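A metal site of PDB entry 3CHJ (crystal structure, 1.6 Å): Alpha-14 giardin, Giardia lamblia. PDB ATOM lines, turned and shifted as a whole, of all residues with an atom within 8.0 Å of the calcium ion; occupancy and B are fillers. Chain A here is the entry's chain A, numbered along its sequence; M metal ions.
The side-chain carboxylate (OE2) of Glu 224 sits close to the indole nitrogen (NE1) of Trp 189, at 3.0 Å. The backbone NH (N) of Lys 182 lies close to the side-chain carboxylate (OE1) of Glu 185, at 3.0 Å. The side-chain carboxylate of Glu 185 is in salt-bridge range of the side-chain amino group of Lys 174 (2.7 Å).
Within 4 Å of the calcium ion: Ala 175, Thr 178, Gly 180, Glu 185 and Glu 224. The nearest printed residue that does not touch the calcium ion is Val 181 (4.2 Å).
The backbone carbonyl oxygen (O) of Ala 175 binds the calcium ion (2.3 Å). OG1 of Thr 178 binds the calcium ion (2.4 Å). O of Gly 180 binds the calcium ion (2.4 Å). The calcium ion is bound by the backbone carbonyl oxygen (O) of Thr 178, at 2.4 Å. The calcium ion is bound by the side-chain carboxylate (OE2) of Glu 224. The calcium ion is bound by OE1 of Glu 224 (2.5 Å). The side-chain carboxylate (OE1) of Glu 185 is bound to the calcium ion. The calcium ion has seven donor atoms within binding distance.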
ATOM      1  N   LEU A 171      27.214 -17.206 -25.661  1.00  0.00           N
ATOM      2  CA  LEU A 171      26.792 -16.304 -26.718  1.00  0.00           C
ATOM      3  C   LEU A 171      25.782 -15.239 -26.246  1.00  0.00           C
ATOM      4  O   LEU A 171      25.917 -14.052 -26.594  1.00  0.00           O
ATOM      5  CB  LEU A 171      26.212 -17.106 -27.896  1.00  0.00           C
ATOM      6  CG  LEU A 171      27.267 -17.896 -28.682  1.00  0.00           C
ATOM      7  CD1 LEU A 171      26.575 -18.881 -29.592  1.00  0.00           C
ATOM      8  CD2 LEU A 171      28.172 -16.952 -29.469  1.00  0.00           C
ATOM      9  N   VAL A 172      24.810 -15.656 -25.437  1.00  0.00           N
ATOM     10  CA  VAL A 172      23.831 -14.694 -24.949  1.00  0.00           C
ATOM     11  C   VAL A 172      24.420 -13.710 -23.911  1.00  0.00           C
ATOM     12  O   VAL A 172      24.056 -12.536 -23.893  1.00  0.00           O
ATOM     13  CB  VAL A 172      22.494 -15.324 -24.488  1.00  0.00           C
ATOM     14  CG1 VAL A 172      22.549 -15.895 -23.049  1.00  0.00           C
ATOM     15  CG2 VAL A 172      21.377 -14.279 -24.635  1.00  0.00           C
ATOM     16  N   ARG A 173      25.343 -14.205 -23.093  1.00  0.00           N
ATOM     17  CA  ARG A 173      26.088 -13.315 -22.210  1.00  0.00           C
ATOM     18  C   ARG A 173      26.861 -12.260 -22.989  1.00  0.00           C
ATOM     19  O   ARG A 173      26.844 -11.076 -22.654  1.00  0.00           O
ATOM     20  CB  ARG A 173      27.029 -14.086 -21.283  1.00  0.00           C
ATOM     21  CG  ARG A 173      27.905 -13.195 -20.431  1.00  0.00           C
ATOM     22  CD  ARG A 173      27.087 -12.447 -19.374  1.00  0.00           C
ATOM     23  NE  ARG A 173      27.948 -11.900 -18.316  1.00  0.00           N
ATOM     24  CZ  ARG A 173      27.509 -11.452 -17.139  1.00  0.00           C
ATOM     25  NH1 ARG A 173      26.213 -11.466 -16.845  1.00  0.00           N
ATOM     26  NH2 ARG A 173      28.365 -10.994 -16.239  1.00  0.00           N
ATOM     27  N   LYS A 174      27.552 -12.688 -24.048  1.00  0.00           N
ATOM     28  CA  LYS A 174      28.260 -11.753 -24.933  1.00  0.00           C
ATOM     29  C   LYS A 174      27.317 -10.681 -25.478  1.00  0.00           C
ATOM     30  O   LYS A 174      27.607  -9.488 -25.421  1.00  0.00           O
ATOM     31  CB  LYS A 174      28.947 -12.533 -26.070  1.00  0.00           C
ATOM     32  CG  LYS A 174      29.829 -11.710 -26.993  1.00  0.00           C
ATOM     33  CD  LYS A 174      29.040 -11.126 -28.162  1.00  0.00           C
ATOM     34  CE  LYS A 174      29.830 -10.069 -28.909  1.00  0.00           C
ATOM     35  NZ  LYS A 174      29.072  -9.518 -30.092  1.00  0.00           N
ATOM     36  N   ALA A 175      26.152 -11.116 -25.947  1.00  0.00           N
ATOM     37  CA  ALA A 175      25.148 -10.207 -26.469  1.00  0.00           C
ATOM     38  C   ALA A 175      24.645  -9.223 -25.416  1.00  0.00           C
ATOM     39  O   ALA A 175      24.473  -8.042 -25.679  1.00  0.00           O
ATOM     40  CB  ALA A 175      23.989 -11.009 -27.065  1.00  0.00           C
ATOM     41  N   ILE A 176      24.419  -9.726 -24.196  1.00  0.00           N
ATOM     42  CA  ILE A 176      23.951  -8.892 -23.104  1.00  0.00           C
ATOM     43  C   ILE A 176      24.985  -7.821 -22.714  1.00  0.00           C
ATOM     44  O   ILE A 176      24.639  -6.698 -22.349  1.00  0.00           O
ATOM     45  CB  ILE A 176      23.555  -9.778 -21.918  1.00  0.00           C
ATOM     46  CG1 ILE A 176      22.221 -10.474 -22.223  1.00  0.00           C
ATOM     47  CG2 ILE A 176      23.485  -8.966 -20.614  1.00  0.00           C
ATOM     48  CD1 ILE A 176      21.848 -11.617 -21.261  1.00  0.00           C
ATOM     49  N   GLU A 177      26.262  -8.187 -22.839  1.00  0.00           N
ATOM     50  CA  GLU A 177      27.328  -7.285 -22.421  1.00  0.00           C
ATOM     51  C   GLU A 177      27.530  -6.096 -23.332  1.00  0.00           C
ATOM     52  O   GLU A 177      27.967  -5.040 -22.873  1.00  0.00           O
ATOM     53  CB  GLU A 177      28.644  -8.038 -22.205  1.00  0.00           C
ATOM     54  CG  GLU A 177      28.648  -8.846 -20.931  1.00  0.00           C
ATOM     55  CD  GLU A 177      30.005  -9.434 -20.582  1.00  0.00           C
ATOM     56  OE1 GLU A 177      31.038  -8.844 -20.958  1.00  0.00           O
ATOM     57  OE2 GLU A 177      30.030 -10.466 -19.898  1.00  0.00           O
ATOM     58  N   THR A 178      27.211  -6.251 -24.621  1.00  0.00           N
ATOM     59  CA  THR A 178      27.397  -5.179 -25.607  1.00  0.00           C
ATOM     60  C   THR A 178      26.167  -4.288 -25.741  1.00  0.00           C
ATOM     61  O   THR A 178      25.032  -4.778 -25.797  1.00  0.00           O
ATOM     62  CB  THR A 178      27.723  -5.736 -27.000  1.00  0.00           C
ATOM     63  OG1 THR A 178      26.620  -6.547 -27.449  1.00  0.00           O
ATOM     64  CG2 THR A 178      29.001  -6.578 -26.981  1.00  0.00           C
ATOM     65  N   LYS A 179      26.394  -2.969 -25.801  1.00  0.00           N
ATOM     66  CA  LYS A 179      25.319  -2.009 -25.993  1.00  0.00           C
ATOM     67  C   LYS A 179      24.708  -2.166 -27.383  1.00  0.00           C
ATOM     68  O   LYS A 179      25.413  -2.097 -28.404  1.00  0.00           O
ATOM     69  CB  LYS A 179      25.831  -0.592 -25.793  1.00  0.00           C
ATOM     70  CG  LYS A 179      24.758   0.482 -25.765  1.00  0.00           C
ATOM     71  CD  LYS A 179      25.370   1.880 -25.744  1.00  0.00           C
ATOM     72  CE  LYS A 179      25.956   2.191 -24.372  1.00  0.00           C
ATOM     73  NZ  LYS A 179      26.604   3.540 -24.314  1.00  0.00           N
ATOM     74  N   GLY A 180      23.399  -2.404 -27.419  1.00  0.00           N
ATOM     75  CA  GLY A 180      22.682  -2.583 -28.691  1.00  0.00           C
ATOM     76  C   GLY A 180      22.828  -4.009 -29.239  1.00  0.00           C
ATOM     77  O   GLY A 180      23.754  -4.736 -28.874  1.00  0.00           O
ATOM     78  N   VAL A 181      21.899  -4.408 -30.115  1.00  0.00           N
ATOM     79  CA  VAL A 181      21.978  -5.714 -30.746  1.00  0.00           C
ATOM     80  C   VAL A 181      22.928  -5.623 -31.920  1.00  0.00           C
ATOM     81  O   VAL A 181      22.623  -4.970 -32.934  1.00  0.00           O
ATOM     82  CB  VAL A 181      20.581  -6.200 -31.236  1.00  0.00           C
ATOM     83  CG1 VAL A 181      20.682  -7.554 -31.920  1.00  0.00           C
ATOM     84  CG2 VAL A 181      19.574  -6.248 -30.073  1.00  0.00           C
ATOM     85  N   LYS A 182      24.089  -6.250 -31.780  1.00  0.00           N
ATOM     86  CA  LYS A 182      25.081  -6.310 -32.862  1.00  0.00           C
ATOM     87  C   LYS A 182      24.655  -7.323 -33.920  1.00  0.00           C
ATOM     88  O   LYS A 182      23.856  -8.220 -33.655  1.00  0.00           O
ATOM     89  CB  LYS A 182      26.471  -6.630 -32.310  1.00  0.00           C
ATOM     90  CG  LYS A 182      26.922  -5.725 -31.160  1.00  0.00           C
ATOM     91  CD  LYS A 182      26.937  -4.268 -31.554  1.00  0.00           C
ATOM     92  CE  LYS A 182      27.586  -3.420 -30.472  1.00  0.00           C
ATOM     93  NZ  LYS A 182      27.518  -1.963 -30.829  1.00  0.00           N
ATOM     94  N   LYS A 183      25.210  -7.183 -35.125  1.00  0.00           N
ATOM     95  CA  LYS A 183      24.838  -8.048 -36.246  1.00  0.00           C
ATOM     96  C   LYS A 183      24.995  -9.538 -35.942  1.00  0.00           C
ATOM     97  O   LYS A 183      24.165 -10.355 -36.369  1.00  0.00           O
ATOM     98  CB  LYS A 183      25.601  -7.649 -37.521  1.00  0.00           C
ATOM     99  CG  LYS A 183      27.111  -7.521 -37.320  1.00  0.00           C
ATOM    100  CD  LYS A 183      27.860  -7.406 -38.657  1.00  0.00           C
ATOM    101  CE  LYS A 183      29.348  -7.587 -38.452  1.00  0.00           C
ATOM    102  NZ  LYS A 183      29.650  -8.828 -37.692  1.00  0.00           N
ATOM    103  N   ASP A 184      26.062  -9.886 -35.211  1.00  0.00           N
ATOM    104  CA  ASP A 184      26.383 -11.274 -34.898  1.00  0.00           C
ATOM    105  C   ASP A 184      25.523 -11.805 -33.746  1.00  0.00           C
ATOM    106  O   ASP A 184      25.515 -13.000 -33.460  1.00  0.00           O
ATOM    107  CB  ASP A 184      27.868 -11.393 -34.512  1.00  0.00           C
ATOM    108  CG  ASP A 184      28.207 -10.636 -33.219  1.00  0.00           C
ATOM    109  OD1 ASP A 184      28.041  -9.401 -33.201  1.00  0.00           O
ATOM    110  OD2 ASP A 184      28.643 -11.274 -32.233  1.00  0.00           O
ATOM    111  N   GLU A 185      24.795 -10.894 -33.093  1.00  0.00           N
ATOM    112  CA  GLU A 185      23.961 -11.252 -31.943  1.00  0.00           C
ATOM    113  C   GLU A 185      22.509 -11.573 -32.312  1.00  0.00           C
ATOM    114  O   GLU A 185      21.798 -12.205 -31.524  1.00  0.00           O
ATOM    115  CB  GLU A 185      24.016 -10.135 -30.903  1.00  0.00           C
ATOM    116  CG  GLU A 185      25.456  -9.914 -30.405  1.00  0.00           C
ATOM    117  CD  GLU A 185      25.671  -8.684 -29.555  1.00  0.00           C
ATOM    118  OE1 GLU A 185      24.735  -7.886 -29.320  1.00  0.00           O
ATOM    119  OE2 GLU A 185      26.837  -8.488 -29.108  1.00  0.00           O
ATOM    120  N   TRP A 189      19.848 -14.305 -30.192  1.00  0.00           N
ATOM    121  CA  TRP A 189      18.598 -13.948 -29.540  1.00  0.00           C
ATOM    122  C   TRP A 189      17.414 -14.694 -30.130  1.00  0.00           C
ATOM    123  O   TRP A 189      16.527 -15.153 -29.406  1.00  0.00           O
ATOM    124  CB  TRP A 189      18.354 -12.457 -29.643  1.00  0.00           C
ATOM    125  CG  TRP A 189      19.188 -11.594 -28.723  1.00  0.00           C
ATOM    126  CD1 TRP A 189      20.156 -10.690 -29.096  1.00  0.00           C
ATOM    127  CD2 TRP A 189      19.103 -11.513 -27.292  1.00  0.00           C
ATOM    128  NE1 TRP A 189      20.658 -10.042 -27.990  1.00  0.00           N
ATOM    129  CE2 TRP A 189      20.056 -10.564 -26.862  1.00  0.00           C
ATOM    130  CE3 TRP A 189      18.316 -12.182 -26.331  1.00  0.00           C
ATOM    131  CZ2 TRP A 189      20.233 -10.229 -25.508  1.00  0.00           C
ATOM    132  CZ3 TRP A 189      18.496 -11.869 -24.974  1.00  0.00           C
ATOM    133  CH2 TRP A 189      19.463 -10.900 -24.581  1.00  0.00           C
ATOM    134  N   GLY A 220      19.118  -8.972 -18.324  1.00  0.00           N
ATOM    135  CA  GLY A 220      19.918  -8.820 -19.537  1.00  0.00           C
ATOM    136  C   GLY A 220      19.060  -8.431 -20.748  1.00  0.00           C
ATOM    137  O   GLY A 220      19.463  -7.626 -21.569  1.00  0.00           O
ATOM    138  N   ASP A 223      18.418  -4.792 -20.400  1.00  0.00           N
ATOM    139  CA  ASP A 223      19.597  -4.036 -20.813  1.00  0.00           C
ATOM    140  C   ASP A 223      19.633  -3.881 -22.334  1.00  0.00           C
ATOM    141  O   ASP A 223      19.892  -2.799 -22.855  1.00  0.00           O
ATOM    142  CB  ASP A 223      20.903  -4.707 -20.360  1.00  0.00           C
ATOM    143  CG  ASP A 223      21.114  -4.660 -18.867  1.00  0.00           C
ATOM    144  OD1 ASP A 223      20.386  -3.930 -18.162  1.00  0.00           O
ATOM    145  OD2 ASP A 223      22.015  -5.369 -18.395  1.00  0.00           O
ATOM    146  N   GLU A 224      19.332  -4.983 -23.020  1.00  0.00           N
ATOM    147  CA  GLU A 224      19.592  -5.087 -24.468  1.00  0.00           C
ATOM    148  C   GLU A 224      18.570  -4.383 -25.345  1.00  0.00           C
ATOM    149  O   GLU A 224      18.917  -3.847 -26.414  1.00  0.00           O
ATOM    150  CB  GLU A 224      19.679  -6.565 -24.879  1.00  0.00           C
ATOM    151  CG  GLU A 224      19.998  -6.811 -26.374  1.00  0.00           C
ATOM    152  CD  GLU A 224      21.474  -6.630 -26.746  1.00  0.00           C
ATOM    153  OE1 GLU A 224      22.146  -5.712 -26.210  1.00  0.00           O
ATOM    154  OE2 GLU A 224      21.975  -7.392 -27.585  1.00  0.00           O
ATOM    155  N   PHE A 225      17.311  -4.425 -24.922  1.00  0.00           N
ATOM    156  CA  PHE A 225      16.212  -4.026 -25.790  1.00  0.00           C
ATOM    157  C   PHE A 225      15.455  -2.857 -25.227  1.00  0.00           C
ATOM    158  O   PHE A 225      15.519  -2.583 -24.033  1.00  0.00           O
ATOM    159  CB  PHE A 225      15.249  -5.190 -25.957  1.00  0.00           C
ATOM    160  CG  PHE A 225      15.848  -6.400 -26.635  1.00  0.00           C
ATOM    161  CD1 PHE A 225      16.091  -6.374 -28.005  1.00  0.00           C
ATOM    162  CD2 PHE A 225      16.161  -7.554 -25.924  1.00  0.00           C
ATOM    163  CE1 PHE A 225      16.628  -7.507 -28.678  1.00  0.00           C
ATOM    164  CE2 PHE A 225      16.708  -8.683 -26.578  1.00  0.00           C
ATOM    165  CZ  PHE A 225      16.944  -8.641 -27.957  1.00  0.00           C
HETATM  166 CA    CA M   1      24.252  -6.490 -27.303  1.00  0.00          CA
